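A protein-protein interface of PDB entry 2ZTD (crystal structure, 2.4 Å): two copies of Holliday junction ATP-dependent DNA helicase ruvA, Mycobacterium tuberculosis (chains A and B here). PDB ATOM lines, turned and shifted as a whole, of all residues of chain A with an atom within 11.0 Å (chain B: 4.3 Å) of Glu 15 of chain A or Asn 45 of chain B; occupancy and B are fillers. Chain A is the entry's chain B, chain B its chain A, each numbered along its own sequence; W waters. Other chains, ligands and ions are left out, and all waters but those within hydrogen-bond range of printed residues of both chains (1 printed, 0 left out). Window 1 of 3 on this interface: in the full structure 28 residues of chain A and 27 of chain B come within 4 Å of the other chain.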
ATOM      1  N   SER A  14       9.115 -26.381   5.176  1.00  0.00           N
ATOM      2  CA  SER A  14      10.206 -25.796   4.408  1.00  0.00           C
ATOM      3  C   SER A  14      11.529 -26.129   5.060  1.00  0.00           C
ATOM      4  O   SER A  14      12.465 -26.531   4.368  1.00  0.00           O
ATOM      5  CB  SER A  14      10.035 -24.291   4.274  1.00  0.00           C
ATOM      6  N   GLU A  15      11.630 -25.982   6.384  1.00  0.00           N
ATOM      7  CA  GLU A  15      12.848 -26.475   7.005  1.00  0.00           C
ATOM      8  C   GLU A  15      12.619 -27.627   7.989  1.00  0.00           C
ATOM      9  O   GLU A  15      11.871 -27.540   8.972  1.00  0.00           O
ATOM     10  CB  GLU A  15      13.674 -25.354   7.599  1.00  0.00           C
ATOM     11  N   PHE A  16      13.266 -28.734   7.667  1.00  0.00           N
ATOM     12  CA  PHE A  16      13.137 -29.983   8.386  1.00  0.00           C
ATOM     13  C   PHE A  16      14.537 -30.528   8.399  1.00  0.00           C
ATOM     14  O   PHE A  16      15.456 -29.903   7.894  1.00  0.00           O
ATOM     15  CB  PHE A  16      12.240 -30.952   7.615  1.00  0.00           C
ATOM     16  CG  PHE A  16      12.453 -30.922   6.117  1.00  0.00           C
ATOM     17  CD1 PHE A  16      13.575 -30.326   5.566  1.00  0.00           C
ATOM     18  CD2 PHE A  16      11.544 -31.507   5.270  1.00  0.00           C
ATOM     19  CE1 PHE A  16      13.770 -30.294   4.203  1.00  0.00           C
ATOM     20  CE2 PHE A  16      11.735 -31.487   3.907  1.00  0.00           C
ATOM     21  CZ  PHE A  16      12.857 -30.873   3.370  1.00  0.00           C
ATOM     22  N   MET A  17      14.700 -31.713   8.941  1.00  0.00           N
ATOM     23  CA  MET A  17      16.022 -32.261   9.145  1.00  0.00           C
ATOM     24  C   MET A  17      16.399 -33.311   8.098  1.00  0.00           C
ATOM     25  O   MET A  17      17.484 -33.243   7.522  1.00  0.00           O
ATOM     26  CB  MET A  17      16.115 -32.823  10.564  1.00  0.00           C
ATOM     27  CG  MET A  17      17.465 -33.364  10.945  1.00  0.00           C
ATOM     28  SD  MET A  17      17.401 -33.916  12.640  1.00  0.00           S
ATOM     29  CE  MET A  17      16.423 -32.590  13.353  1.00  0.00           C
ATOM     30  N   ILE A  18      15.519 -34.287   7.854  1.00  0.00           N
ATOM     31  CA  ILE A  18      15.855 -35.379   6.934  1.00  0.00           C
ATOM     32  C   ILE A  18      15.431 -35.078   5.484  1.00  0.00           C
ATOM     33  O   ILE A  18      14.253 -35.107   5.117  1.00  0.00           O
ATOM     34  CB  ILE A  18      15.348 -36.754   7.395  1.00  0.00           C
ATOM     35  CG1 ILE A  18      15.829 -37.041   8.818  1.00  0.00           C
ATOM     36  CG2 ILE A  18      15.858 -37.844   6.448  1.00  0.00           C
ATOM     37  CD1 ILE A  18      15.627 -38.469   9.272  1.00  0.00           C
ATOM     38  N   ALA A  19      16.431 -34.793   4.670  1.00  0.00           N
ATOM     39  CA  ALA A  19      16.203 -34.267   3.340  1.00  0.00           C
ATOM     40  C   ALA A  19      16.272 -35.366   2.295  1.00  0.00           C
ATOM     41  O   ALA A  19      15.811 -35.175   1.172  1.00  0.00           O
ATOM     42  CB  ALA A  19      17.213 -33.179   3.044  1.00  0.00           C
ATOM     43  N   THR A  64      13.272 -36.518   0.582  1.00  0.00           N
ATOM     44  CA  THR A  64      12.188 -36.635   1.562  1.00  0.00           C
ATOM     45  C   THR A  64      11.737 -35.330   2.215  1.00  0.00           C
ATOM     46  O   THR A  64      12.487 -34.373   2.294  1.00  0.00           O
ATOM     47  CB  THR A  64      12.567 -37.634   2.675  1.00  0.00           C
ATOM     48  OG1 THR A  64      13.808 -37.229   3.280  1.00  0.00           O
ATOM     49  CG2 THR A  64      12.709 -39.063   2.098  1.00  0.00           C
ATOM     50  N   ALA A  65      10.489 -35.307   2.661  1.00  0.00           N
ATOM     51  CA  ALA A  65       9.989 -34.259   3.536  1.00  0.00           C
ATOM     52  C   ALA A  65       9.746 -34.914   4.874  1.00  0.00           C
ATOM     53  O   ALA A  65       9.074 -35.934   4.943  1.00  0.00           O
ATOM     54  CB  ALA A  65       8.693 -33.655   3.005  1.00  0.00           C
ATOM     55  N   MET A  66      10.326 -34.356   5.931  1.00  0.00           N
ATOM     56  CA  MET A  66      10.143 -34.919   7.259  1.00  0.00           C
ATOM     57  C   MET A  66       8.999 -34.185   7.957  1.00  0.00           C
ATOM     58  O   MET A  66       9.000 -32.958   8.053  1.00  0.00           O
ATOM     59  CB  MET A  66      11.437 -34.827   8.060  1.00  0.00           C
ATOM     60  CG  MET A  66      11.287 -35.319   9.480  1.00  0.00           C
ATOM     61  SD  MET A  66      12.834 -35.854  10.231  1.00  0.00           S
ATOM     62  CE  MET A  66      12.383 -35.703  11.942  1.00  0.00           C
ATOM     63  N   ILE A  67       7.998 -34.936   8.420  1.00  0.00           N
ATOM     64  CA  ILE A  67       6.880 -34.295   9.100  1.00  0.00           C
ATOM     65  C   ILE A  67       6.800 -34.630  10.585  1.00  0.00           C
ATOM     66  O   ILE A  67       6.729 -35.794  10.973  1.00  0.00           O
ATOM     67  CB  ILE A  67       5.555 -34.549   8.405  1.00  0.00           C
ATOM     68  CG1 ILE A  67       5.673 -34.100   6.939  1.00  0.00           C
ATOM     69  CG2 ILE A  67       4.434 -33.811   9.140  1.00  0.00           C
ATOM     70  CD1 ILE A  67       4.404 -33.586   6.363  1.00  0.00           C
ATOM     71  N   VAL A  68       6.842 -33.581  11.401  1.00  0.00           N
ATOM     72  CA  VAL A  68       6.917 -33.724  12.840  1.00  0.00           C
ATOM     73  C   VAL A  68       5.662 -33.170  13.491  1.00  0.00           C
ATOM     74  O   VAL A  68       5.344 -31.984  13.357  1.00  0.00           O
ATOM     75  CB  VAL A  68       8.130 -32.982  13.409  1.00  0.00           C
ATOM     76  CG1 VAL A  68       8.002 -32.843  14.923  1.00  0.00           C
ATOM     77  CG2 VAL A  68       9.416 -33.691  13.025  1.00  0.00           C
ATOM     78  N   ARG A  69       4.947 -34.036  14.181  1.00  0.00           N
ATOM     79  CA  ARG A  69       3.793 -33.627  14.956  1.00  0.00           C
ATOM     80  C   ARG A  69       3.980 -34.162  16.374  1.00  0.00           C
ATOM     81  O   ARG A  69       4.811 -35.045  16.603  1.00  0.00           O
ATOM     82  CB  ARG A  69       2.494 -34.156  14.320  1.00  0.00           C
ATOM     83  CG  ARG A  69       2.213 -33.644  12.901  1.00  0.00           C
ATOM     84  CD  ARG A  69       2.207 -32.107  12.797  1.00  0.00           C
ATOM     85  NE  ARG A  69       2.021 -31.637  11.422  1.00  0.00           N
ATOM     86  CZ  ARG A  69       3.000 -31.194  10.629  1.00  0.00           C
ATOM     87  NH1 ARG A  69       4.253 -31.155  11.072  1.00  0.00           N
ATOM     88  NH2 ARG A  69       2.728 -30.790   9.390  1.00  0.00           N
ATOM     89  N   THR A  74       7.198 -38.553  10.455  1.00  0.00           N
ATOM     90  CA  THR A  74       6.971 -39.262   9.190  1.00  0.00           C
ATOM     91  C   THR A  74       7.816 -38.725   8.043  1.00  0.00           C
ATOM     92  O   THR A  74       8.004 -37.505   7.897  1.00  0.00           O
ATOM     93  CB  THR A  74       5.485 -39.184   8.728  1.00  0.00           C
ATOM     94  OG1 THR A  74       4.607 -39.244   9.856  1.00  0.00           O
ATOM     95  CG2 THR A  74       5.161 -40.310   7.753  1.00  0.00           C
ATOM     96  N   LEU A  75       8.321 -39.642   7.226  1.00  0.00           N
ATOM     97  CA  LEU A  75       9.042 -39.291   6.019  1.00  0.00           C
ATOM     98  C   LEU A  75       8.171 -39.544   4.797  1.00  0.00           C
ATOM     99  O   LEU A  75       7.576 -40.636   4.652  1.00  0.00           O
ATOM    100  CB  LEU A  75      10.345 -40.090   5.912  1.00  0.00           C
ATOM    101  CG  LEU A  75      11.407 -39.759   6.976  1.00  0.00           C
ATOM    102  CD1 LEU A  75      12.519 -40.790   7.014  1.00  0.00           C
ATOM    103  CD2 LEU A  75      11.994 -38.380   6.745  1.00  0.00           C
ATOM    104  N   ARG A  84       9.464 -33.114  -4.189  1.00  0.00           N
ATOM    105  CA  ARG A  84       9.383 -32.962  -2.734  1.00  0.00           C
ATOM    106  C   ARG A  84       8.929 -31.547  -2.361  1.00  0.00           C
ATOM    107  O   ARG A  84       8.130 -31.377  -1.436  1.00  0.00           O
ATOM    108  CB  ARG A  84      10.725 -33.293  -2.066  1.00  0.00           C
ATOM    109  CG  ARG A  84      10.680 -33.418  -0.538  1.00  0.00           C
ATOM    110  CD  ARG A  84      10.918 -32.074   0.156  1.00  0.00           C
ATOM    111  NE  ARG A  84      11.985 -31.314  -0.499  1.00  0.00           N
ATOM    112  CZ  ARG A  84      13.286 -31.559  -0.359  1.00  0.00           C
ATOM    113  NH1 ARG A  84      13.704 -32.559   0.419  1.00  0.00           N
ATOM    114  NH2 ARG A  84      14.174 -30.811  -1.007  1.00  0.00           N
ATOM    115  N   ASP A  85       9.427 -30.536  -3.080  1.00  0.00           N
ATOM    116  CA  ASP A  85       9.079 -29.149  -2.759  1.00  0.00           C
ATOM    117  C   ASP A  85       7.613 -28.885  -3.122  1.00  0.00           C
ATOM    118  O   ASP A  85       6.906 -28.133  -2.451  1.00  0.00           O
ATOM    119  CB  ASP A  85      10.010 -28.148  -3.471  1.00  0.00           C
ATOM    120  CG  ASP A  85      11.456 -28.174  -2.945  1.00  0.00           C
ATOM    121  OD1 ASP A  85      12.309 -27.448  -3.510  1.00  0.00           O
ATOM    122  OD2 ASP A  85      11.738 -28.920  -1.971  1.00  0.00           O
ATOM    123  N   LEU A  88       5.483 -30.146  -0.175  1.00  0.00           N
ATOM    124  CA  LEU A  88       5.487 -29.130   0.888  1.00  0.00           C
ATOM    125  C   LEU A  88       4.582 -27.946   0.534  1.00  0.00           C
ATOM    126  O   LEU A  88       3.852 -27.421   1.378  1.00  0.00           O
ATOM    127  CB  LEU A  88       6.907 -28.615   1.130  1.00  0.00           C
ATOM    128  CG  LEU A  88       7.924 -29.626   1.637  1.00  0.00           C
ATOM    129  CD1 LEU A  88       9.351 -29.064   1.545  1.00  0.00           C
ATOM    130  CD2 LEU A  88       7.550 -30.044   3.046  1.00  0.00           C
ATOM    131  N   THR A  89       4.640 -27.539  -0.723  1.00  0.00           N
ATOM    132  CA  THR A  89       3.784 -26.472  -1.219  1.00  0.00           C
ATOM    133  C   THR A  89       2.294 -26.789  -1.046  1.00  0.00           C
ATOM    134  O   THR A  89       1.531 -25.962  -0.555  1.00  0.00           O
ATOM    135  CB  THR A  89       4.123 -26.161  -2.678  1.00  0.00           C
ATOM    136  OG1 THR A  89       5.465 -25.656  -2.743  1.00  0.00           O
ATOM    137  CG2 THR A  89       3.165 -25.129  -3.261  1.00  0.00           C
ATOM    138  N   LEU A  91       1.006 -28.666   1.204  1.00  0.00           N
ATOM    139  CA  LEU A  91       0.743 -28.562   2.647  1.00  0.00           C
ATOM    140  C   LEU A  91       0.525 -27.118   3.127  1.00  0.00           C
ATOM    141  O   LEU A  91      -0.028 -26.905   4.202  1.00  0.00           O
ATOM    142  CB  LEU A  91       1.863 -29.228   3.472  1.00  0.00           C
ATOM    143  CG  LEU A  91       2.187 -30.680   3.096  1.00  0.00           C
ATOM    144  CD1 LEU A  91       3.438 -31.174   3.777  1.00  0.00           C
ATOM    145  CD2 LEU A  91       1.020 -31.564   3.424  1.00  0.00           C
ATOM    146  N   ALA A 170      16.499 -14.783  -2.054  1.00  0.00           N
ATOM    147  CA  ALA A 170      17.222 -15.164  -0.855  1.00  0.00           C
ATOM    148  C   ALA A 170      17.192 -14.012   0.121  1.00  0.00           C
ATOM    149  O   ALA A 170      16.995 -14.192   1.328  1.00  0.00           O
ATOM    150  CB  ALA A 170      18.646 -15.524  -1.203  1.00  0.00           C
ATOM    151  N   GLY A 173      13.801 -13.534   1.445  1.00  0.00           N
ATOM    152  CA  GLY A 173      13.590 -14.588   2.407  1.00  0.00           C
ATOM    153  C   GLY A 173      14.217 -14.232   3.735  1.00  0.00           C
ATOM    154  O   GLY A 173      13.671 -14.535   4.795  1.00  0.00           O
ATOM    155  N   LEU A 174      15.368 -13.585   3.677  1.00  0.00           N
ATOM    156  CA  LEU A 174      16.044 -13.124   4.875  1.00  0.00           C
ATOM    157  C   LEU A 174      15.321 -11.952   5.531  1.00  0.00           C
ATOM    158  O   LEU A 174      15.655 -11.548   6.644  1.00  0.00           O
ATOM    159  CB  LEU A 174      17.469 -12.723   4.538  1.00  0.00           C
ATOM    160  CG  LEU A 174      18.372 -13.917   4.270  1.00  0.00           C
ATOM    161  CD1 LEU A 174      19.668 -13.469   3.601  1.00  0.00           C
ATOM    162  CD2 LEU A 174      18.626 -14.667   5.577  1.00  0.00           C
ATOM    163  N   ASP B  31      20.494 -20.933   1.241  1.00  0.00           N
ATOM    164  CA  ASP B  31      20.143 -20.762   2.644  1.00  0.00           C
ATOM    165  C   ASP B  31      20.233 -22.086   3.407  1.00  0.00           C
ATOM    166  O   ASP B  31      19.666 -22.228   4.489  1.00  0.00           O
ATOM    167  CB  ASP B  31      18.731 -20.197   2.753  1.00  0.00           C
ATOM    168  CG  ASP B  31      17.700 -21.103   2.138  1.00  0.00           C
ATOM    169  OD1 ASP B  31      18.086 -22.160   1.611  1.00  0.00           O
ATOM    170  OD2 ASP B  31      16.506 -20.755   2.181  1.00  0.00           O
ATOM    171  N   HIS B  32      20.926 -23.057   2.826  1.00  0.00           N
ATOM    172  CA  HIS B  32      21.053 -24.360   3.462  1.00  0.00           C
ATOM    173  C   HIS B  32      21.915 -25.247   2.588  1.00  0.00           C
ATOM    174  O   HIS B  32      22.180 -24.944   1.430  1.00  0.00           O
ATOM    175  CB  HIS B  32      19.681 -25.018   3.680  1.00  0.00           C
ATOM    176  CG  HIS B  32      19.060 -25.523   2.416  1.00  0.00           C
ATOM    177  ND1 HIS B  32      18.082 -24.823   1.739  1.00  0.00           N
ATOM    178  CD2 HIS B  32      19.251 -26.673   1.728  1.00  0.00           C
ATOM    179  CE1 HIS B  32      17.705 -25.518   0.679  1.00  0.00           C
ATOM    180  NE2 HIS B  32      18.404 -26.636   0.647  1.00  0.00           N
ATOM    181  N   ARG B  43      19.412 -31.761   6.122  1.00  0.00           N
ATOM    182  CA  ARG B  43      19.308 -30.375   5.750  1.00  0.00           C
ATOM    183  C   ARG B  43      19.744 -29.512   6.926  1.00  0.00           C
ATOM    184  O   ARG B  43      19.163 -29.578   8.017  1.00  0.00           O
ATOM    185  CB  ARG B  43      17.884 -30.026   5.359  1.00  0.00           C
ATOM    186  CG  ARG B  43      17.719 -28.561   4.982  1.00  0.00           C
ATOM    187  CD  ARG B  43      16.270 -28.127   5.052  1.00  0.00           C
ATOM    188  NE  ARG B  43      16.148 -26.689   4.871  1.00  0.00           N
ATOM    189  CZ  ARG B  43      15.850 -26.110   3.712  1.00  0.00           C
ATOM    190  NH1 ARG B  43      15.629 -26.860   2.636  1.00  0.00           N
ATOM    191  NH2 ARG B  43      15.774 -24.789   3.630  1.00  0.00           N
ATOM    192  N   VAL B  44      20.786 -28.726   6.712  1.00  0.00           N
ATOM    193  CA  VAL B  44      21.189 -27.760   7.712  1.00  0.00           C
ATOM    194  C   VAL B  44      21.197 -26.361   7.121  1.00  0.00           C
ATOM    195  O   VAL B  44      21.806 -26.102   6.093  1.00  0.00           O
ATOM    196  CB  VAL B  44      22.507 -28.162   8.489  1.00  0.00           C
ATOM    197  CG1 VAL B  44      22.315 -29.434   9.306  1.00  0.00           C
ATOM    198  CG2 VAL B  44      23.712 -28.226   7.580  1.00  0.00           C
ATOM    199  N   ASN B  45      20.455 -25.484   7.771  1.00  0.00           N
ATOM    200  CA  ASN B  45      20.366 -24.097   7.352  1.00  0.00           C
ATOM    201  C   ASN B  45      21.600 -23.313   7.766  1.00  0.00           C
ATOM    202  O   ASN B  45      22.149 -23.532   8.855  1.00  0.00           O
ATOM    203  CB  ASN B  45      19.083 -23.480   7.899  1.00  0.00           C
ATOM    204  CG  ASN B  45      17.853 -24.134   7.314  1.00  0.00           C
ATOM    205  OD1 ASN B  45      17.729 -25.358   7.302  1.00  0.00           O
ATOM    206  ND2 ASN B  45      16.908 -23.318   6.869  1.00  0.00           N
ATOM    207  N   ALA B  46      22.056 -22.437   6.882  1.00  0.00           N
ATOM    208  CA  ALA B  46      23.341 -21.775   7.074  1.00  0.00           C
ATOM    209  C   ALA B  46      23.367 -20.430   6.360  1.00  0.00           C
ATOM    210  O   ALA B  46      22.608 -20.210   5.416  1.00  0.00           O
ATOM    211  CB  ALA B  46      24.465 -22.671   6.578  1.00  0.00           C
ATOM    212  N   THR B  74      14.837 -28.770  13.412  1.00  0.00           N
ATOM    213  CA  THR B  74      15.702 -28.089  12.445  1.00  0.00           C
ATOM    214  C   THR B  74      17.156 -27.990  12.891  1.00  0.00           C
ATOM    215  O   THR B  74      17.437 -27.756  14.074  1.00  0.00           O
ATOM    216  CB  THR B  74      15.198 -26.652  12.193  1.00  0.00           C
ATOM    217  OG1 THR B  74      13.764 -26.637  12.213  1.00  0.00           O
ATOM    218  CG2 THR B  74      15.708 -26.129  10.864  1.00  0.00           C
ATOM    219  N   LEU B  75      18.069 -28.168  11.939  1.00  0.00           N
ATOM    220  CA  LEU B  75      19.488 -27.936  12.169  1.00  0.00           C
ATOM    221  C   LEU B  75      19.922 -26.589  11.580  1.00  0.00           C
ATOM    222  O   LEU B  75      19.618 -26.259  10.417  1.00  0.00           O
ATOM    223  CB  LEU B  75      20.328 -29.078  11.585  1.00  0.00           C
ATOM    224  CG  LEU B  75      20.123 -30.442  12.252  1.00  0.00           C
ATOM    225  CD1 LEU B  75      20.690 -31.556  11.389  1.00  0.00           C
ATOM    226  CD2 LEU B  75      20.725 -30.500  13.640  1.00  0.00           C
ATOM    227  N   TYR B  76      20.611 -25.794  12.400  1.00  0.00           N
ATOM    228  CA  TYR B  76      21.307 -24.604  11.909  1.00  0.00           C
ATOM    229  C   TYR B  76      22.794 -24.855  12.065  1.00  0.00           C
ATOM    230  O   TYR B  76      23.247 -25.311  13.111  1.00  0.00           O
ATOM    231  CB  TYR B  76      20.876 -23.365  12.689  1.00  0.00           C
ATOM    232  CG  TYR B  76      19.389 -23.132  12.638  1.00  0.00           C
ATOM    233  CD1 TYR B  76      18.841 -22.249  11.716  1.00  0.00           C
ATOM    234  CD2 TYR B  76      18.525 -23.812  13.486  1.00  0.00           C
ATOM    235  CE1 TYR B  76      17.477 -22.049  11.646  1.00  0.00           C
ATOM    236  CE2 TYR B  76      17.164 -23.609  13.431  1.00  0.00           C
ATOM    237  CZ  TYR B  76      16.651 -22.720  12.507  1.00  0.00           C
ATOM    238  OH  TYR B  76      15.303 -22.512  12.440  1.00  0.00           O
ATOM    239  N   GLY B  77      23.551 -24.573  11.007  1.00  0.00           N
ATOM    240  CA  GLY B  77      24.960 -24.929  10.970  1.00  0.00           C
ATOM    241  C   GLY B  77      25.899 -23.784  10.690  1.00  0.00           C
ATOM    242  O   GLY B  77      25.524 -22.786  10.063  1.00  0.00           O
ATOM    243  N   MET B 102      19.422 -16.132  12.243  1.00  0.00           N
ATOM    244  CA  MET B 102      20.108 -16.473  10.991  1.00  0.00           C
ATOM    245  C   MET B 102      20.185 -15.253  10.102  1.00  0.00           C
ATOM    246  O   MET B 102      21.242 -14.950   9.541  1.00  0.00           O
ATOM    247  CB  MET B 102      19.397 -17.613  10.264  1.00  0.00           C
ATOM    248  CG  MET B 102      19.432 -18.942  11.012  1.00  0.00           C
ATOM    249  SD  MET B 102      21.098 -19.602  11.171  1.00  0.00           S
ATOM    250  CE  MET B 102      21.610 -19.588   9.440  1.00  0.00           C
HETATM  251  O   HOH W   1      17.042 -28.502   9.090  1.00  0.00           O
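Water W1 lies within hydrogen-bond range of the backbone carbonyl oxygen of Phe 16 of chain A (2.4 Å), the backbone carbonyl oxygen of Arg 43 of chain B (2.6 Å) and the backbone NH of Leu 75 of chain B (3.0 Å).
Glu 15 of chain A touches three residues of chain B.
Printed residues of chain B within 4 Å of Met 17 of chain A: Arg 43 (2.8 Å) and Leu 75 (3.7 Å).
No residue of chain A comes within 4 Å of Asp 31 of chain B.
Arg 43 of chain B touches just these residues of chain A: Ser 14 (3.5 Å), Glu 15 (3.9 Å), Phe 16 (3.4 Å), Met 17 (2.8 Å) and Ala 19 (3.97 Å).
Of chain A, only Glu 15 (3.9 Å) comes within 4 Å of Asn 45 of chain B.
Printed residues of chain A within 4 Å of Thr 74 of chain B: Glu 15.
Tyr 76 of chain B touches none of the printed residues of chain A.
No residue of chain A comes within 4 Å of Gly 77 of chain B.
The nearest printed residue of chain B that does not touch Glu 15 of chain A is Tyr 76 of chain B (5.8 Å).
The nearest residue of chain A that does not touch Asn 45 of chain B is Phe 16 of chain A (5.1 Å).
Among the printed residues, no Asp or Glu carboxylate lies within 4 Å of a Lys or Arg side-chain nitrogen of the other chain.
NH2 of Arg 43 of chain B is in hydrogen-bond range of ND1 of His 32 of chain B (3.0 Å).
The guanidinium group (NE) of Arg 43 of chain B lies within hydrogen-bond range of the side-chain amide oxygen (OD1) of Asn 45 of chain B (3.2 Å).
The backbone carbonyl oxygen (O) of Ala 19 of chain A lies within hydrogen-bond range of the guanidinium group (NH1) of Arg 84 of chain A (3.4 Å).
N of Asn 45 of chain B sits at hydrogen-bond distance from O of Leu 75 of chain B, 2.9 Å away.
The backbone NH of Thr 64 of chain A is in hydrogen-bond range of the backbone carbonyl oxygen of Ala 19 of chain A (2.9 Å).
The backbone carbonyl oxygen of Asn 45 of chain B lies within hydrogen-bond range of the backbone NH of Gly 77 of chain B (2.8 Å).
Ser 14 of chain A touches Arg 43 of chain B (O to CZ, 3.5 Å).
CB of Glu 15 of chain A touches NE of Arg 43 of chain B, at 3.9 Å.
Glu 15 of chain A touches Asn 45 of chain B (CB to ND2, 3.9 Å).
Thr 74 of chain B touches Glu 15 of chain A (OG1 to O, 3.9 Å).
CD of Arg 43 of chain B touches CE1 of Phe 16 of chain A, 3.4 Å away.
CG of Met 17 of chain A touches CD1 of Leu 75 of chain B, at 3.7 Å.
CB of Ala 19 of chain A touches CB of Arg 43 of chain B, 3.97 Å away.
2 positions are printed for both chains.
O of Met 17 of chain A lies within hydrogen-bond range of N of Arg 43 of chain B (2.8 Å).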
